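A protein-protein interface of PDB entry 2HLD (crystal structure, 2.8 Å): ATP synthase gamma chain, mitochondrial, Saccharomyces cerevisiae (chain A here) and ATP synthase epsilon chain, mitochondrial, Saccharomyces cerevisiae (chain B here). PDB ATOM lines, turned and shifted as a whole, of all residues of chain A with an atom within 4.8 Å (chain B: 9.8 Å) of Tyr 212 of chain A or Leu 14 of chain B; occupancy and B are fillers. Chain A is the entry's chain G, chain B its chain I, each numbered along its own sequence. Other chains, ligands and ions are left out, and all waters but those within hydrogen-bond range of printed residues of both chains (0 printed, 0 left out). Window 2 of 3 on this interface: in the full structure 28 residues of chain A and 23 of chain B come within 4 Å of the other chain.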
ATOM      1  N   MET A  44     -16.738 -17.623 -14.430  1.00  0.00           N
ATOM      2  CA  MET A  44     -15.761 -18.530 -15.034  1.00  0.00           C
ATOM      3  C   MET A  44     -14.398 -17.843 -15.216  1.00  0.00           C
ATOM      4  O   MET A  44     -13.372 -18.499 -15.394  1.00  0.00           O
ATOM      5  CB  MET A  44     -16.276 -19.035 -16.376  1.00  0.00           C
ATOM      6  CG  MET A  44     -15.639 -20.317 -16.837  1.00  0.00           C
ATOM      7  SD  MET A  44     -15.938 -20.442 -18.582  1.00  0.00           S
ATOM      8  CE  MET A  44     -15.645 -22.165 -18.969  1.00  0.00           C
ATOM      9  N   GLU A  48     -11.272 -19.683 -13.597  1.00  0.00           N
ATOM     10  CA  GLU A  48     -10.150 -19.925 -14.506  1.00  0.00           C
ATOM     11  C   GLU A  48      -8.876 -19.170 -14.099  1.00  0.00           C
ATOM     12  O   GLU A  48      -7.772 -19.696 -14.213  1.00  0.00           O
ATOM     13  CB  GLU A  48     -10.572 -19.534 -15.932  1.00  0.00           C
ATOM     14  CG  GLU A  48      -9.507 -19.653 -17.017  1.00  0.00           C
ATOM     15  CD  GLU A  48      -9.332 -21.074 -17.537  1.00  0.00           C
ATOM     16  OE1 GLU A  48      -9.941 -22.019 -16.967  1.00  0.00           O
ATOM     17  OE2 GLU A  48      -8.577 -21.241 -18.525  1.00  0.00           O
ATOM     18  N   ASP A 208      -1.908 -26.555 -23.248  1.00  0.00           N
ATOM     19  CA  ASP A 208      -3.363 -26.589 -23.289  1.00  0.00           C
ATOM     20  C   ASP A 208      -3.962 -25.564 -22.359  1.00  0.00           C
ATOM     21  O   ASP A 208      -4.944 -24.916 -22.706  1.00  0.00           O
ATOM     22  CB  ASP A 208      -3.889 -27.978 -22.928  1.00  0.00           C
ATOM     23  CG  ASP A 208      -3.404 -29.053 -23.882  1.00  0.00           C
ATOM     24  OD1 ASP A 208      -3.266 -28.776 -25.110  1.00  0.00           O
ATOM     25  OD2 ASP A 208      -3.140 -30.211 -23.472  1.00  0.00           O
ATOM     26  N   LEU A 209      -3.370 -25.417 -21.178  1.00  0.00           N
ATOM     27  CA  LEU A 209      -3.813 -24.422 -20.219  1.00  0.00           C
ATOM     28  C   LEU A 209      -3.639 -22.993 -20.776  1.00  0.00           C
ATOM     29  O   LEU A 209      -4.071 -22.020 -20.154  1.00  0.00           O
ATOM     30  CB  LEU A 209      -3.059 -24.612 -18.906  1.00  0.00           C
ATOM     31  CG  LEU A 209      -3.445 -23.849 -17.631  1.00  0.00           C
ATOM     32  CD1 LEU A 209      -4.935 -23.989 -17.310  1.00  0.00           C
ATOM     33  CD2 LEU A 209      -2.579 -24.277 -16.425  1.00  0.00           C
ATOM     34  N   PHE A 210      -3.011 -22.880 -21.954  1.00  0.00           N
ATOM     35  CA  PHE A 210      -2.841 -21.602 -22.657  1.00  0.00           C
ATOM     36  C   PHE A 210      -3.818 -21.514 -23.811  1.00  0.00           C
ATOM     37  O   PHE A 210      -4.503 -20.500 -23.949  1.00  0.00           O
ATOM     38  CB  PHE A 210      -1.374 -21.370 -23.120  1.00  0.00           C
ATOM     39  CG  PHE A 210      -1.232 -20.605 -24.437  1.00  0.00           C
ATOM     40  CD1 PHE A 210      -1.463 -19.229 -24.506  1.00  0.00           C
ATOM     41  CD2 PHE A 210      -0.854 -21.274 -25.608  1.00  0.00           C
ATOM     42  CE1 PHE A 210      -1.337 -18.534 -25.736  1.00  0.00           C
ATOM     43  CE2 PHE A 210      -0.715 -20.582 -26.839  1.00  0.00           C
ATOM     44  CZ  PHE A 210      -0.953 -19.219 -26.901  1.00  0.00           C
ATOM     45  N   GLU A 211      -3.884 -22.554 -24.639  1.00  0.00           N
ATOM     46  CA  GLU A 211      -4.827 -22.556 -25.755  1.00  0.00           C
ATOM     47  C   GLU A 211      -6.283 -22.452 -25.284  1.00  0.00           C
ATOM     48  O   GLU A 211      -7.108 -21.824 -25.927  1.00  0.00           O
ATOM     49  CB  GLU A 211      -4.624 -23.766 -26.656  1.00  0.00           C
ATOM     50  CG  GLU A 211      -3.299 -23.752 -27.402  1.00  0.00           C
ATOM     51  CD  GLU A 211      -3.194 -24.846 -28.454  1.00  0.00           C
ATOM     52  OE1 GLU A 211      -3.736 -25.953 -28.232  1.00  0.00           O
ATOM     53  OE2 GLU A 211      -2.558 -24.607 -29.508  1.00  0.00           O
ATOM     54  N   TYR A 212      -6.573 -23.040 -24.134  1.00  0.00           N
ATOM     55  CA  TYR A 212      -7.888 -22.967 -23.514  1.00  0.00           C
ATOM     56  C   TYR A 212      -8.153 -21.584 -22.913  1.00  0.00           C
ATOM     57  O   TYR A 212      -9.294 -21.102 -22.931  1.00  0.00           O
ATOM     58  CB  TYR A 212      -7.974 -24.045 -22.435  1.00  0.00           C
ATOM     59  CG  TYR A 212      -9.258 -24.106 -21.654  1.00  0.00           C
ATOM     60  CD1 TYR A 212     -10.352 -24.848 -22.124  1.00  0.00           C
ATOM     61  CD2 TYR A 212      -9.373 -23.463 -20.419  1.00  0.00           C
ATOM     62  CE1 TYR A 212     -11.533 -24.933 -21.389  1.00  0.00           C
ATOM     63  CE2 TYR A 212     -10.552 -23.528 -19.682  1.00  0.00           C
ATOM     64  CZ  TYR A 212     -11.624 -24.271 -20.168  1.00  0.00           C
ATOM     65  OH  TYR A 212     -12.783 -24.354 -19.431  1.00  0.00           O
ATOM     66  N   THR A 213      -7.112 -20.969 -22.353  1.00  0.00           N
ATOM     67  CA  THR A 213      -7.220 -19.616 -21.809  1.00  0.00           C
ATOM     68  C   THR A 213      -7.331 -18.563 -22.931  1.00  0.00           C
ATOM     69  O   THR A 213      -8.046 -17.556 -22.787  1.00  0.00           O
ATOM     70  CB  THR A 213      -6.055 -19.327 -20.877  1.00  0.00           C
ATOM     71  OG1 THR A 213      -5.994 -20.362 -19.895  1.00  0.00           O
ATOM     72  CG2 THR A 213      -6.334 -18.105 -20.024  1.00  0.00           C
ATOM     73  N   LEU A 214      -6.672 -18.824 -24.062  1.00  0.00           N
ATOM     74  CA  LEU A 214      -6.826 -17.958 -25.209  1.00  0.00           C
ATOM     75  C   LEU A 214      -8.316 -17.824 -25.519  1.00  0.00           C
ATOM     76  O   LEU A 214      -8.842 -16.704 -25.565  1.00  0.00           O
ATOM     77  CB  LEU A 214      -6.024 -18.444 -26.426  1.00  0.00           C
ATOM     78  CG  LEU A 214      -5.790 -17.337 -27.470  1.00  0.00           C
ATOM     79  CD1 LEU A 214      -5.132 -16.130 -26.815  1.00  0.00           C
ATOM     80  CD2 LEU A 214      -4.990 -17.795 -28.693  1.00  0.00           C
ATOM     81  N   ALA A 215      -8.996 -18.961 -25.690  1.00  0.00           N
ATOM     82  CA  ALA A 215     -10.439 -18.992 -25.971  1.00  0.00           C
ATOM     83  C   ALA A 215     -11.281 -18.434 -24.822  1.00  0.00           C
ATOM     84  O   ALA A 215     -12.032 -17.494 -25.007  1.00  0.00           O
ATOM     85  CB  ALA A 215     -10.863 -20.372 -26.307  1.00  0.00           C
ATOM     86  N   ASN A 216     -11.139 -18.976 -23.628  1.00  0.00           N
ATOM     87  CA  ASN A 216     -11.935 -18.491 -22.508  1.00  0.00           C
ATOM     88  C   ASN A 216     -11.842 -17.007 -22.227  1.00  0.00           C
ATOM     89  O   ASN A 216     -12.851 -16.367 -21.956  1.00  0.00           O
ATOM     90  CB  ASN A 216     -11.586 -19.253 -21.238  1.00  0.00           C
ATOM     91  CG  ASN A 216     -12.381 -20.507 -21.099  1.00  0.00           C
ATOM     92  OD1 ASN A 216     -13.143 -20.649 -20.151  1.00  0.00           O
ATOM     93  ND2 ASN A 216     -12.229 -21.430 -22.058  1.00  0.00           N
ATOM     94  N   ILE B   8      -5.623 -28.187 -35.798  1.00  0.00           N
ATOM     95  CA  ILE B   8      -6.768 -27.859 -34.900  1.00  0.00           C
ATOM     96  C   ILE B   8      -6.300 -27.792 -33.437  1.00  0.00           C
ATOM     97  O   ILE B   8      -5.526 -28.643 -32.999  1.00  0.00           O
ATOM     98  CB  ILE B   8      -7.933 -28.876 -35.091  1.00  0.00           C
ATOM     99  N   SER B   9      -6.773 -26.781 -32.698  1.00  0.00           N
ATOM    100  CA  SER B   9      -6.310 -26.495 -31.324  1.00  0.00           C
ATOM    101  C   SER B   9      -7.115 -27.182 -30.214  1.00  0.00           C
ATOM    102  O   SER B   9      -8.152 -27.784 -30.485  1.00  0.00           O
ATOM    103  CB  SER B   9      -6.282 -24.983 -31.086  1.00  0.00           C
ATOM    104  OG  SER B   9      -7.437 -24.344 -31.617  1.00  0.00           O
ATOM    105  N   TYR B  10      -6.635 -27.078 -28.971  1.00  0.00           N
ATOM    106  CA  TYR B  10      -7.302 -27.694 -27.804  1.00  0.00           C
ATOM    107  C   TYR B  10      -8.703 -27.143 -27.507  1.00  0.00           C
ATOM    108  O   TYR B  10      -9.553 -27.869 -27.001  1.00  0.00           O
ATOM    109  CB  TYR B  10      -6.418 -27.632 -26.541  1.00  0.00           C
ATOM    110  CG  TYR B  10      -7.068 -28.171 -25.258  1.00  0.00           C
ATOM    111  CD1 TYR B  10      -7.262 -29.544 -25.057  1.00  0.00           C
ATOM    112  CD2 TYR B  10      -7.477 -27.301 -24.239  1.00  0.00           C
ATOM    113  CE1 TYR B  10      -7.860 -30.033 -23.876  1.00  0.00           C
ATOM    114  CE2 TYR B  10      -8.071 -27.781 -23.061  1.00  0.00           C
ATOM    115  CZ  TYR B  10      -8.256 -29.143 -22.883  1.00  0.00           C
ATOM    116  OH  TYR B  10      -8.846 -29.605 -21.718  1.00  0.00           O
ATOM    117  N   ALA B  11      -8.942 -25.869 -27.811  1.00  0.00           N
ATOM    118  CA  ALA B  11     -10.258 -25.269 -27.591  1.00  0.00           C
ATOM    119  C   ALA B  11     -11.166 -25.474 -28.807  1.00  0.00           C
ATOM    120  O   ALA B  11     -12.396 -25.409 -28.695  1.00  0.00           O
ATOM    121  CB  ALA B  11     -10.119 -23.798 -27.263  1.00  0.00           C
ATOM    122  N   ALA B  12     -10.546 -25.701 -29.965  1.00  0.00           N
ATOM    123  CA  ALA B  12     -11.268 -26.069 -31.174  1.00  0.00           C
ATOM    124  C   ALA B  12     -11.735 -27.519 -31.035  1.00  0.00           C
ATOM    125  O   ALA B  12     -12.873 -27.849 -31.374  1.00  0.00           O
ATOM    126  CB  ALA B  12     -10.382 -25.893 -32.398  1.00  0.00           C
ATOM    127  N   TYR B  13     -10.843 -28.370 -30.522  1.00  0.00           N
ATOM    128  CA  TYR B  13     -11.165 -29.758 -30.200  1.00  0.00           C
ATOM    129  C   TYR B  13     -12.296 -29.823 -29.164  1.00  0.00           C
ATOM    130  O   TYR B  13     -13.304 -30.489 -29.398  1.00  0.00           O
ATOM    131  CB  TYR B  13      -9.892 -30.540 -29.778  1.00  0.00           C
ATOM    132  CG  TYR B  13     -10.067 -31.567 -28.667  1.00  0.00           C
ATOM    133  CD1 TYR B  13     -10.022 -31.174 -27.328  1.00  0.00           C
ATOM    134  CD2 TYR B  13     -10.256 -32.924 -28.948  1.00  0.00           C
ATOM    135  CE1 TYR B  13     -10.182 -32.091 -26.284  1.00  0.00           C
ATOM    136  CE2 TYR B  13     -10.412 -33.865 -27.900  1.00  0.00           C
ATOM    137  CZ  TYR B  13     -10.376 -33.429 -26.567  1.00  0.00           C
ATOM    138  OH  TYR B  13     -10.524 -34.297 -25.501  1.00  0.00           O
ATOM    139  N   LEU B  14     -12.145 -29.109 -28.048  1.00  0.00           N
ATOM    140  CA  LEU B  14     -13.205 -29.017 -27.041  1.00  0.00           C
ATOM    141  C   LEU B  14     -14.532 -28.484 -27.595  1.00  0.00           C
ATOM    142  O   LEU B  14     -15.597 -28.883 -27.126  1.00  0.00           O
ATOM    143  CB  LEU B  14     -12.774 -28.148 -25.861  1.00  0.00           C
ATOM    144  CG  LEU B  14     -12.045 -28.754 -24.663  1.00  0.00           C
ATOM    145  CD1 LEU B  14     -12.182 -27.788 -23.490  1.00  0.00           C
ATOM    146  CD2 LEU B  14     -12.563 -30.142 -24.275  1.00  0.00           C
ATOM    147  N   ASN B  15     -14.452 -27.581 -28.575  1.00  0.00           N
ATOM    148  CA  ASN B  15     -15.626 -27.023 -29.246  1.00  0.00           C
ATOM    149  C   ASN B  15     -16.433 -28.114 -29.950  1.00  0.00           C
ATOM    150  O   ASN B  15     -17.650 -28.235 -29.751  1.00  0.00           O
ATOM    151  CB  ASN B  15     -15.205 -25.943 -30.253  1.00  0.00           C
ATOM    152  CG  ASN B  15     -16.336 -25.536 -31.207  1.00  0.00           C
ATOM    153  OD1 ASN B  15     -16.257 -25.760 -32.419  1.00  0.00           O
ATOM    154  ND2 ASN B  15     -17.389 -24.936 -30.659  1.00  0.00           N
ATOM    155  N   VAL B  16     -15.734 -28.902 -30.765  1.00  0.00           N
ATOM    156  CA  VAL B  16     -16.334 -30.007 -31.506  1.00  0.00           C
ATOM    157  C   VAL B  16     -16.989 -31.029 -30.562  1.00  0.00           C
ATOM    158  O   VAL B  16     -18.079 -31.530 -30.847  1.00  0.00           O
ATOM    159  CB  VAL B  16     -15.291 -30.647 -32.476  1.00  0.00           C
ATOM    160  CG1 VAL B  16     -15.501 -32.157 -32.637  1.00  0.00           C
ATOM    161  CG2 VAL B  16     -15.319 -29.927 -33.842  1.00  0.00           C
ATOM    162  N   ALA B  17     -16.331 -31.293 -29.430  1.00  0.00           N
ATOM    163  CA  ALA B  17     -16.834 -32.204 -28.391  1.00  0.00           C
ATOM    164  C   ALA B  17     -18.012 -31.610 -27.613  1.00  0.00           C
ATOM    165  O   ALA B  17     -18.708 -32.323 -26.893  1.00  0.00           O
ATOM    166  CB  ALA B  17     -15.704 -32.597 -27.430  1.00  0.00           C
ATOM    167  N   ALA B  18     -18.214 -30.301 -27.752  1.00  0.00           N
ATOM    168  CA  ALA B  18     -19.337 -29.604 -27.130  1.00  0.00           C
ATOM    169  C   ALA B  18     -20.457 -29.396 -28.142  1.00  0.00           C
ATOM    170  O   ALA B  18     -21.604 -29.141 -27.755  1.00  0.00           O
ATOM    171  CB  ALA B  18     -18.883 -28.263 -26.538  1.00  0.00           C
ATOM    172  N   GLN B  19     -20.116 -29.502 -29.430  1.00  0.00           N
ATOM    173  CA  GLN B  19     -21.093 -29.325 -30.510  1.00  0.00           C
ATOM    174  C   GLN B  19     -21.711 -30.641 -30.947  1.00  0.00           C
ATOM    175  O   GLN B  19     -22.804 -30.653 -31.523  1.00  0.00           O
ATOM    176  CB  GLN B  19     -20.496 -28.621 -31.734  1.00  0.00           C
ATOM    177  CG  GLN B  19     -21.545 -27.822 -32.526  1.00  0.00           C
ATOM    178  CD  GLN B  19     -21.382 -27.919 -34.038  1.00  0.00           C
ATOM    179  OE1 GLN B  19     -20.361 -28.399 -34.534  1.00  0.00           O
ATOM    180  NE2 GLN B  19     -22.395 -27.465 -34.771  1.00  0.00           N
ATOM    181  N   ALA B  20     -20.995 -31.739 -30.700  1.00  0.00           N
ATOM    182  CA  ALA B  20     -21.558 -33.073 -30.870  1.00  0.00           C
ATOM    183  C   ALA B  20     -22.564 -33.288 -29.742  1.00  0.00           C
ATOM    184  O   ALA B  20     -23.758 -33.428 -30.007  1.00  0.00           O
ATOM    185  CB  ALA B  20     -20.472 -34.141 -30.871  1.00  0.00           C
ATOM    186  N   ILE B  21     -22.093 -33.261 -28.496  1.00  0.00           N
ATOM    187  CA  ILE B  21     -22.983 -33.290 -27.320  1.00  0.00           C
ATOM    188  C   ILE B  21     -24.088 -32.201 -27.350  1.00  0.00           C
ATOM    189  O   ILE B  21     -24.911 -32.095 -26.438  1.00  0.00           O
ATOM    190  CB  ILE B  21     -22.162 -33.232 -26.003  1.00  0.00           C
ATOM    191  N   ARG B  22     -24.091 -31.390 -28.401  1.00  0.00           N
ATOM    192  CA  ARG B  22     -25.234 -30.544 -28.690  1.00  0.00           C
ATOM    193  C   ARG B  22     -26.130 -31.338 -29.639  1.00  0.00           C
ATOM    194  O   ARG B  22     -27.085 -31.978 -29.189  1.00  0.00           O
ATOM    195  CB  ARG B  22     -24.799 -29.201 -29.289  1.00  0.00           C
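OE1 of Glu 211 of chain A sits at hydrogen-bond distance from N of Tyr 10 of chain B (3.2 Å).
The side-chain amide nitrogen of Asn 216 of chain A lies within hydrogen-bond range of the backbone carbonyl oxygen of Tyr 212 of chain A (3.1 Å).
Tyr 10 of chain B touches Asp 208 of chain A (CB to OD1, 3.6 Å). OE1 of Glu 211 of chain A touches CB of Ser 9 of chain B, 3.9 Å away. Glu 211 of chain A touches Ala 11 of chain B (O to CB, 3.8 Å). Tyr 10 of chain B touches Tyr 212 of chain A (CD2 to CB, 3.8 Å). Leu 14 of chain B touches Tyr 212 of chain A. Ala 215 of chain A touches Ala 11 of chain B (CB to CB, 3.6 Å).
Printed residues of chain B within 4 Å of Tyr 212 of chain A: Tyr 10 (3.8 Å) and Leu 14 (3.6 Å). Leu 14 of chain B touches just one residue of chain A: Tyr 212. Ala 215 of chain A touches one residue of chain B. Of the printed residues of chain A, Ala 11 of chain B touches Glu 211 and Ala 215. Of the printed residues of chain A, Tyr 10 of chain B touches Asp 208, Glu 211 and Tyr 212. Of the printed residues of chain B, Glu 211 of chain A touches Ser 9 (3.9 Å), Tyr 10 (3.2 Å) and Ala 11 (3.8 Å). Printed residues of chain A within 4 Å of Ser 9 of chain B: Glu 211 (3.9 Å). Asn 216 of chain A touches none of the printed residues of chain B. The nearest printed residue of chain A that does not touch Leu 14 of chain B is Asn 216 of chain A (6.5 Å). The nearest printed residue of chain B that does not touch Glu 211 of chain A is Ile 8 of chain B (5.8 Å).
Of the 15 printed residues of chain B, 4 touch a printed residue of chain A. Hydrophobic or aromatic side chains of chain B that line the printed part of chain A: Tyr 10, Ala 11 and Leu 14. Of the 11 printed residues of chain A, 4 touch a printed residue of chain B. Printed residues of chain A that touch a printed residue of chain B: Asp 208, Glu 211, Tyr 212 and Ala 215. Hydrophobic or aromatic side chains of chain A within 4 Å of the printed part of chain B: Tyr 212 and Ala 215. Among the printed residues, no Asp or Glu carboxylate lies within 4 Å of a Lys or Arg side-chain nitrogen of the other chain.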
